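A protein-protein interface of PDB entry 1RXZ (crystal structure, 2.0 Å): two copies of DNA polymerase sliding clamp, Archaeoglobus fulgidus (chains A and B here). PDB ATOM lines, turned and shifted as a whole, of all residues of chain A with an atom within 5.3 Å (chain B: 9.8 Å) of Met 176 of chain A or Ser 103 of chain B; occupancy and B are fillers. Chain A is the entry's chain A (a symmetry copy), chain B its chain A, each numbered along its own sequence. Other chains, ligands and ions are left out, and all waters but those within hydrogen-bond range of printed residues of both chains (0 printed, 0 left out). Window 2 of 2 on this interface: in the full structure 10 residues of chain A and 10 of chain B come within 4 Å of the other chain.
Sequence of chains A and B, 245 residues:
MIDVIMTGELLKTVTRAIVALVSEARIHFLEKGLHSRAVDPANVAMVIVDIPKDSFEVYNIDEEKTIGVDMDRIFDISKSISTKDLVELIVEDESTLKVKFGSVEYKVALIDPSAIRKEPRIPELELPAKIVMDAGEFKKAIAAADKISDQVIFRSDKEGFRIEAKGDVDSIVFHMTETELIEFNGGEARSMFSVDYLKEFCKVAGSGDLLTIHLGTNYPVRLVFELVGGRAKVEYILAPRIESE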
ATOM      1  N   MET A 133     -18.634  11.366   6.449  1.00  0.00           N
ATOM      2  CA  MET A 133     -18.744  10.775   7.768  1.00  0.00           C
ATOM      3  C   MET A 133     -17.350  10.512   8.308  1.00  0.00           C
ATOM      4  O   MET A 133     -16.349  10.806   7.655  1.00  0.00           O
ATOM      5  CB  MET A 133     -19.526   9.450   7.699  1.00  0.00           C
ATOM      6  CG  MET A 133     -18.732   8.270   7.111  1.00  0.00           C
ATOM      7  SD  MET A 133     -19.670   6.713   6.949  1.00  0.00           S
ATOM      8  CE  MET A 133     -19.562   6.038   8.603  1.00  0.00           C
ATOM      9  N   GLU A 137     -16.350   5.336  12.180  1.00  0.00           N
ATOM     10  CA  GLU A 137     -17.716   4.850  12.130  1.00  0.00           C
ATOM     11  C   GLU A 137     -17.867   3.983  10.890  1.00  0.00           C
ATOM     12  O   GLU A 137     -18.618   3.010  10.893  1.00  0.00           O
ATOM     13  CB  GLU A 137     -18.689   6.032  12.049  1.00  0.00           C
ATOM     14  CG  GLU A 137     -19.326   6.432  13.368  1.00  0.00           C
ATOM     15  CD  GLU A 137     -20.279   5.377  13.892  1.00  0.00           C
ATOM     16  OE1 GLU A 137     -19.803   4.306  14.318  1.00  0.00           O
ATOM     17  OE2 GLU A 137     -21.506   5.613  13.869  1.00  0.00           O
ATOM     18  N   GLU A 159     -33.522   9.543   3.439  1.00  0.00           N
ATOM     19  CA  GLU A 159     -33.559   9.094   4.826  1.00  0.00           C
ATOM     20  C   GLU A 159     -32.201   8.672   5.386  1.00  0.00           C
ATOM     21  O   GLU A 159     -32.133   8.026   6.428  1.00  0.00           O
ATOM     22  CB  GLU A 159     -34.546   7.933   4.984  1.00  0.00           C
ATOM     23  CG  GLU A 159     -34.855   7.583   6.438  1.00  0.00           C
ATOM     24  CD  GLU A 159     -35.453   6.201   6.595  1.00  0.00           C
ATOM     25  OE1 GLU A 159     -36.501   5.933   5.973  1.00  0.00           O
ATOM     26  OE2 GLU A 159     -34.872   5.384   7.344  1.00  0.00           O
ATOM     27  N   GLY A 160     -31.120   9.026   4.702  1.00  0.00           N
ATOM     28  CA  GLY A 160     -29.812   8.665   5.214  1.00  0.00           C
ATOM     29  C   GLY A 160     -28.990   7.741   4.346  1.00  0.00           C
ATOM     30  O   GLY A 160     -29.411   7.324   3.265  1.00  0.00           O
ATOM     31  N   PHE A 161     -27.794   7.432   4.834  1.00  0.00           N
ATOM     32  CA  PHE A 161     -26.858   6.557   4.142  1.00  0.00           C
ATOM     33  C   PHE A 161     -26.936   5.167   4.759  1.00  0.00           C
ATOM     34  O   PHE A 161     -26.952   5.030   5.979  1.00  0.00           O
ATOM     35  CB  PHE A 161     -25.437   7.117   4.277  1.00  0.00           C
ATOM     36  CG  PHE A 161     -24.373   6.234   3.701  1.00  0.00           C
ATOM     37  CD1 PHE A 161     -24.447   5.795   2.389  1.00  0.00           C
ATOM     38  CD2 PHE A 161     -23.290   5.842   4.476  1.00  0.00           C
ATOM     39  CE1 PHE A 161     -23.460   4.977   1.859  1.00  0.00           C
ATOM     40  CE2 PHE A 161     -22.300   5.025   3.957  1.00  0.00           C
ATOM     41  CZ  PHE A 161     -22.386   4.590   2.643  1.00  0.00           C
ATOM     42  N   VAL A 173     -27.178  -3.924   9.136  1.00  0.00           N
ATOM     43  CA  VAL A 173     -27.333  -2.665   8.418  1.00  0.00           C
ATOM     44  C   VAL A 173     -26.783  -1.516   9.239  1.00  0.00           C
ATOM     45  O   VAL A 173     -27.080  -1.375  10.430  1.00  0.00           O
ATOM     46  CB  VAL A 173     -28.808  -2.341   8.078  1.00  0.00           C
ATOM     47  CG1 VAL A 173     -28.873  -1.082   7.229  1.00  0.00           C
ATOM     48  CG2 VAL A 173     -29.442  -3.484   7.335  1.00  0.00           C
ATOM     49  N   PHE A 174     -25.969  -0.703   8.572  1.00  0.00           N
ATOM     50  CA  PHE A 174     -25.346   0.483   9.149  1.00  0.00           C
ATOM     51  C   PHE A 174     -26.062   1.702   8.565  1.00  0.00           C
ATOM     52  O   PHE A 174     -25.893   2.022   7.390  1.00  0.00           O
ATOM     53  CB  PHE A 174     -23.874   0.525   8.761  1.00  0.00           C
ATOM     54  CG  PHE A 174     -23.178   1.762   9.200  1.00  0.00           C
ATOM     55  CD1 PHE A 174     -22.602   1.837  10.463  1.00  0.00           C
ATOM     56  CD2 PHE A 174     -23.111   2.865   8.358  1.00  0.00           C
ATOM     57  CE1 PHE A 174     -21.970   2.989  10.885  1.00  0.00           C
ATOM     58  CE2 PHE A 174     -22.480   4.029   8.768  1.00  0.00           C
ATOM     59  CZ  PHE A 174     -21.904   4.093  10.036  1.00  0.00           C
ATOM     60  N   HIS A 175     -26.862   2.376   9.388  1.00  0.00           N
ATOM     61  CA  HIS A 175     -27.626   3.535   8.937  1.00  0.00           C
ATOM     62  C   HIS A 175     -27.325   4.785   9.727  1.00  0.00           C
ATOM     63  O   HIS A 175     -27.184   4.738  10.943  1.00  0.00           O
ATOM     64  CB  HIS A 175     -29.129   3.260   9.035  1.00  0.00           C
ATOM     65  CG  HIS A 175     -29.991   4.363   8.493  1.00  0.00           C
ATOM     66  ND1 HIS A 175     -31.341   4.457   8.766  1.00  0.00           N
ATOM     67  CD2 HIS A 175     -29.708   5.395   7.659  1.00  0.00           C
ATOM     68  CE1 HIS A 175     -31.851   5.494   8.127  1.00  0.00           C
ATOM     69  NE2 HIS A 175     -30.880   6.080   7.447  1.00  0.00           N
ATOM     70  N   MET A 176     -27.234   5.903   9.012  1.00  0.00           N
ATOM     71  CA  MET A 176     -26.981   7.213   9.595  1.00  0.00           C
ATOM     72  C   MET A 176     -27.778   8.254   8.826  1.00  0.00           C
ATOM     73  O   MET A 176     -27.453   8.575   7.685  1.00  0.00           O
ATOM     74  CB  MET A 176     -25.500   7.564   9.525  1.00  0.00           C
ATOM     75  CG  MET A 176     -24.628   6.717  10.419  1.00  0.00           C
ATOM     76  SD  MET A 176     -22.921   7.266  10.380  1.00  0.00           S
ATOM     77  CE  MET A 176     -22.717   7.861  12.056  1.00  0.00           C
ATOM     78  N   THR A 177     -28.834   8.763   9.452  1.00  0.00           N
ATOM     79  CA  THR A 177     -29.672   9.775   8.823  1.00  0.00           C
ATOM     80  C   THR A 177     -28.783  10.967   8.514  1.00  0.00           C
ATOM     81  O   THR A 177     -27.686  11.077   9.063  1.00  0.00           O
ATOM     82  CB  THR A 177     -30.804  10.224   9.761  1.00  0.00           C
ATOM     83  OG1 THR A 177     -30.254  10.977  10.849  1.00  0.00           O
ATOM     84  CG2 THR A 177     -31.545   9.012  10.310  1.00  0.00           C
ATOM     85  N   GLU A 178     -29.245  11.855   7.636  1.00  0.00           N
ATOM     86  CA  GLU A 178     -28.442  13.019   7.280  1.00  0.00           C
ATOM     87  C   GLU A 178     -28.126  13.834   8.530  1.00  0.00           C
ATOM     88  O   GLU A 178     -27.124  14.555   8.585  1.00  0.00           O
ATOM     89  CB  GLU A 178     -29.174  13.893   6.258  1.00  0.00           C
ATOM     90  CG  GLU A 178     -30.386  14.615   6.792  1.00  0.00           C
ATOM     91  CD  GLU A 178     -30.937  15.616   5.798  1.00  0.00           C
ATOM     92  OE1 GLU A 178     -30.128  16.399   5.249  1.00  0.00           O
ATOM     93  OE2 GLU A 178     -32.172  15.627   5.572  1.00  0.00           O
ATOM     94  N   GLU A 180     -27.170  12.729  11.353  1.00  0.00           N
ATOM     95  CA  GLU A 180     -26.015  12.198  12.072  1.00  0.00           C
ATOM     96  C   GLU A 180     -24.748  12.132  11.221  1.00  0.00           C
ATOM     97  O   GLU A 180     -23.663  11.816  11.714  1.00  0.00           O
ATOM     98  CB  GLU A 180     -26.342  10.818  12.663  1.00  0.00           C
ATOM     99  CG  GLU A 180     -27.364  10.000  11.893  1.00  0.00           C
ATOM    100  CD  GLU A 180     -27.706   8.704  12.601  1.00  0.00           C
ATOM    101  OE1 GLU A 180     -28.591   7.972  12.103  1.00  0.00           O
ATOM    102  OE2 GLU A 180     -27.092   8.416  13.654  1.00  0.00           O
ATOM    103  N   LEU A 181     -24.889  12.437   9.938  1.00  0.00           N
ATOM    104  CA  LEU A 181     -23.749  12.445   9.035  1.00  0.00           C
ATOM    105  C   LEU A 181     -23.153  13.840   9.091  1.00  0.00           C
ATOM    106  O   LEU A 181     -23.869  14.814   9.361  1.00  0.00           O
ATOM    107  CB  LEU A 181     -24.191  12.166   7.597  1.00  0.00           C
ATOM    108  CG  LEU A 181     -24.502  10.736   7.173  1.00  0.00           C
ATOM    109  CD1 LEU A 181     -25.115  10.750   5.784  1.00  0.00           C
ATOM    110  CD2 LEU A 181     -23.218   9.908   7.206  1.00  0.00           C
ATOM    111  N   ILE B  81     -19.570  -5.213  18.921  1.00  0.00           N
ATOM    112  CA  ILE B  81     -20.173  -4.486  20.024  1.00  0.00           C
ATOM    113  C   ILE B  81     -19.043  -4.046  20.932  1.00  0.00           C
ATOM    114  O   ILE B  81     -18.229  -4.863  21.352  1.00  0.00           O
ATOM    115  CB  ILE B  81     -21.113  -5.403  20.827  1.00  0.00           C
ATOM    116  CG1 ILE B  81     -22.003  -6.197  19.871  1.00  0.00           C
ATOM    117  CG2 ILE B  81     -21.959  -4.578  21.783  1.00  0.00           C
ATOM    118  CD1 ILE B  81     -22.892  -7.214  20.557  1.00  0.00           C
ATOM    119  N   SER B  82     -18.990  -2.757  21.234  1.00  0.00           N
ATOM    120  CA  SER B  82     -17.935  -2.232  22.084  1.00  0.00           C
ATOM    121  C   SER B  82     -18.235  -2.444  23.564  1.00  0.00           C
ATOM    122  O   SER B  82     -19.365  -2.762  23.938  1.00  0.00           O
ATOM    123  CB  SER B  82     -17.735  -0.750  21.781  1.00  0.00           C
ATOM    124  OG  SER B  82     -17.516  -0.561  20.391  1.00  0.00           O
ATOM    125  N   ASP B  85     -20.293   0.485  24.394  1.00  0.00           N
ATOM    126  CA  ASP B  85     -21.379   0.602  23.432  1.00  0.00           C
ATOM    127  C   ASP B  85     -22.607  -0.148  23.929  1.00  0.00           C
ATOM    128  O   ASP B  85     -22.725  -1.359  23.732  1.00  0.00           O
ATOM    129  CB  ASP B  85     -20.938   0.027  22.078  1.00  0.00           C
ATOM    130  CG  ASP B  85     -21.982   0.213  20.985  1.00  0.00           C
ATOM    131  OD1 ASP B  85     -21.791  -0.354  19.884  1.00  0.00           O
ATOM    132  OD2 ASP B  85     -22.983   0.925  21.220  1.00  0.00           O
ATOM    133  N   LEU B  86     -23.512   0.574  24.588  1.00  0.00           N
ATOM    134  CA  LEU B  86     -24.740  -0.028  25.086  1.00  0.00           C
ATOM    135  C   LEU B  86     -25.349  -0.831  23.950  1.00  0.00           C
ATOM    136  O   LEU B  86     -25.319  -0.413  22.793  1.00  0.00           O
ATOM    137  CB  LEU B  86     -25.741   1.050  25.523  1.00  0.00           C
ATOM    138  CG  LEU B  86     -25.523   1.806  26.839  1.00  0.00           C
ATOM    139  CD1 LEU B  86     -25.786   0.885  28.025  1.00  0.00           C
ATOM    140  CD2 LEU B  86     -24.109   2.366  26.876  1.00  0.00           C
ATOM    141  N   GLU B  88     -28.888  -2.961  22.761  1.00  0.00           N
ATOM    142  CA  GLU B  88     -30.279  -3.241  23.066  1.00  0.00           C
ATOM    143  C   GLU B  88     -30.745  -4.477  22.305  1.00  0.00           C
ATOM    144  O   GLU B  88     -30.657  -4.541  21.079  1.00  0.00           O
ATOM    145  CB  GLU B  88     -31.170  -2.041  22.712  1.00  0.00           C
ATOM    146  CG  GLU B  88     -31.329  -1.778  21.219  1.00  0.00           C
ATOM    147  CD  GLU B  88     -32.334  -0.666  20.904  1.00  0.00           C
ATOM    148  OE1 GLU B  88     -33.517  -0.788  21.305  1.00  0.00           O
ATOM    149  OE2 GLU B  88     -31.941   0.327  20.248  1.00  0.00           O
ATOM    150  N   VAL B  99     -30.094  -6.915  17.340  1.00  0.00           N
ATOM    151  CA  VAL B  99     -29.048  -6.520  18.261  1.00  0.00           C
ATOM    152  C   VAL B  99     -28.608  -5.150  17.763  1.00  0.00           C
ATOM    153  O   VAL B  99     -28.079  -5.024  16.656  1.00  0.00           O
ATOM    154  CB  VAL B  99     -27.862  -7.515  18.230  1.00  0.00           C
ATOM    155  CG1 VAL B  99     -26.932  -7.255  19.405  1.00  0.00           C
ATOM    156  CG2 VAL B  99     -28.380  -8.942  18.267  1.00  0.00           C
ATOM    157  N   LYS B 100     -28.852  -4.124  18.576  1.00  0.00           N
ATOM    158  CA  LYS B 100     -28.505  -2.753  18.213  1.00  0.00           C
ATOM    159  C   LYS B 100     -27.388  -2.175  19.068  1.00  0.00           C
ATOM    160  O   LYS B 100     -27.376  -2.342  20.283  1.00  0.00           O
ATOM    161  CB  LYS B 100     -29.754  -1.873  18.299  1.00  0.00           C
ATOM    162  CG  LYS B 100     -30.891  -2.425  17.459  1.00  0.00           C
ATOM    163  CD  LYS B 100     -32.150  -1.609  17.551  1.00  0.00           C
ATOM    164  CE  LYS B 100     -33.246  -2.298  16.752  1.00  0.00           C
ATOM    165  NZ  LYS B 100     -34.523  -1.519  16.740  1.00  0.00           N
ATOM    166  N   PHE B 101     -26.446  -1.502  18.417  1.00  0.00           N
ATOM    167  CA  PHE B 101     -25.312  -0.898  19.101  1.00  0.00           C
ATOM    168  C   PHE B 101     -24.602   0.066  18.164  1.00  0.00           C
ATOM    169  O   PHE B 101     -24.038  -0.336  17.148  1.00  0.00           O
ATOM    170  CB  PHE B 101     -24.342  -1.987  19.584  1.00  0.00           C
ATOM    171  CG  PHE B 101     -23.946  -2.980  18.517  1.00  0.00           C
ATOM    172  CD1 PHE B 101     -22.730  -2.854  17.841  1.00  0.00           C
ATOM    173  CD2 PHE B 101     -24.791  -4.045  18.189  1.00  0.00           C
ATOM    174  CE1 PHE B 101     -22.360  -3.777  16.852  1.00  0.00           C
ATOM    175  CE2 PHE B 101     -24.434  -4.972  17.204  1.00  0.00           C
ATOM    176  CZ  PHE B 101     -23.217  -4.839  16.535  1.00  0.00           C
ATOM    177  N   GLY B 102     -24.621   1.345  18.514  1.00  0.00           N
ATOM    178  CA  GLY B 102     -24.000   2.335  17.660  1.00  0.00           C
ATOM    179  C   GLY B 102     -24.943   2.556  16.495  1.00  0.00           C
ATOM    180  O   GLY B 102     -26.152   2.716  16.703  1.00  0.00           O
ATOM    181  N   SER B 103     -24.406   2.556  15.274  1.00  0.00           N
ATOM    182  CA  SER B 103     -25.220   2.752  14.070  1.00  0.00           C
ATOM    183  C   SER B 103     -25.506   1.428  13.367  1.00  0.00           C
ATOM    184  O   SER B 103     -25.971   1.402  12.231  1.00  0.00           O
ATOM    185  CB  SER B 103     -24.517   3.707  13.102  1.00  0.00           C
ATOM    186  OG  SER B 103     -24.410   5.006  13.661  1.00  0.00           O
ATOM    187  N   VAL B 104     -25.226   0.329  14.060  1.00  0.00           N
ATOM    188  CA  VAL B 104     -25.453  -1.004  13.520  1.00  0.00           C
ATOM    189  C   VAL B 104     -26.608  -1.729  14.196  1.00  0.00           C
ATOM    190  O   VAL B 104     -26.759  -1.704  15.419  1.00  0.00           O
ATOM    191  CB  VAL B 104     -24.197  -1.894  13.667  1.00  0.00           C
ATOM    192  CG1 VAL B 104     -24.500  -3.306  13.190  1.00  0.00           C
ATOM    193  CG2 VAL B 104     -23.049  -1.313  12.864  1.00  0.00           C
ATOM    194  N   GLU B 105     -27.432  -2.358  13.371  1.00  0.00           N
ATOM    195  CA  GLU B 105     -28.552  -3.156  13.839  1.00  0.00           C
ATOM    196  C   GLU B 105     -28.378  -4.498  13.158  1.00  0.00           C
ATOM    197  O   GLU B 105     -28.559  -4.617  11.950  1.00  0.00           O
ATOM    198  CB  GLU B 105     -29.890  -2.549  13.432  1.00  0.00           C
ATOM    199  CG  GLU B 105     -31.063  -3.461  13.726  1.00  0.00           C
ATOM    200  CD  GLU B 105     -32.401  -2.875  13.291  1.00  0.00           C
ATOM    201  OE1 GLU B 105     -33.325  -3.664  12.989  1.00  0.00           O
ATOM    202  OE2 GLU B 105     -32.536  -1.629  13.260  1.00  0.00           O
ATOM    203  N   TYR B 106     -27.990  -5.494  13.942  1.00  0.00           N
ATOM    204  CA  TYR B 106     -27.779  -6.843  13.446  1.00  0.00           C
ATOM    205  C   TYR B 106     -29.037  -7.668  13.712  1.00  0.00           C
ATOM    206  O   TYR B 106     -29.641  -7.582  14.778  1.00  0.00           O
ATOM    207  CB  TYR B 106     -26.568  -7.449  14.157  1.00  0.00           C
ATOM    208  CG  TYR B 106     -26.338  -8.925  13.933  1.00  0.00           C
ATOM    209  CD1 TYR B 106     -26.102  -9.432  12.662  1.00  0.00           C
ATOM    210  CD2 TYR B 106     -26.278  -9.803  15.014  1.00  0.00           C
ATOM    211  CE1 TYR B 106     -25.803 -10.782  12.472  1.00  0.00           C
ATOM    212  CE2 TYR B 106     -25.980 -11.153  14.839  1.00  0.00           C
ATOM    213  CZ  TYR B 106     -25.739 -11.640  13.567  1.00  0.00           C
ATOM    214  OH  TYR B 106     -25.419 -12.974  13.394  1.00  0.00           O
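The backbone NH of His 175 of chain A lies within hydrogen-bond range of the backbone carbonyl oxygen of Ser 103 of chain B (3.1 Å). The side-chain hydroxyl (OG) of Ser 103 of chain B lies within hydrogen-bond range of the side-chain carboxylate (OE2) of Glu 137 of chain A. The backbone carbonyl oxygen of Ser 103 of chain B lies close to the backbone carbonyl oxygen of Val 173 of chain A (3.5 Å). O of Val 173 of chain A is in hydrogen-bond range of N of Glu 105 of chain B (3.1 Å).
The backbone carbonyl oxygen (O) of Glu 159 of chain A sits at hydrogen-bond distance from a ring nitrogen (NE2) of His 175 of chain A (2.5 Å). The backbone NH (N) of Phe 161 of chain A sits at hydrogen-bond distance from the backbone carbonyl oxygen (O) of Met 176 of chain A, 3.1 Å away.
Printed residues of chain B that touch a printed residue of chain A: Ser 103, Val 104 and Glu 105. Among the printed residues, 8 pairs touch across the chains. Among the printed residues, no Asp or Glu carboxylate lies within 4 Å of a Lys or Arg side-chain nitrogen of the other chain.
Of the printed residues of chain B, Glu 137 of chain A touches Ser 103 (3.0 Å). Printed residues of chain B within 4 Å of Val 173 of chain A: Ser 103, Val 104 and Glu 105. Of the printed residues of chain B, Phe 174 of chain A touches Ser 103 and Val 104. Of chain B, only Ser 103 comes within 4 Å of His 175 of chain A. Met 176 of chain A touches just one residue of chain B: Ser 103 (3.7 Å). Asp 85 of chain B touches none of the printed residues of chain A. Phe 101 of chain B touches none of the printed residues of chain A. Ser 103 of chain B touches just these residues of chain A: Glu 137 (3.0 Å), Val 173 (3.5 Å), Phe 174 (3.3 Å), His 175 (3.1 Å) and Met 176 (3.7 Å). Of the printed residues of chain A, Val 104 of chain B touches Val 173 and Phe 174. The nearest residue of chain B that does not touch Met 176 of chain A is Gly 102 of chain B (7.3 Å). The nearest residue of chain A that does not touch Ser 103 of chain B is Glu 180 of chain A (4.3 Å).
Val 173 of chain A touches Val 104 of chain B. Ser 103 of chain B touches Phe 174 of chain A (O to CA, 3.3 Å). Phe 174 of chain A touches Val 104 of chain B. Met 176 of chain A touches Ser 103 of chain B (CG to OG, 3.7 Å).
No position is printed for both chains.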
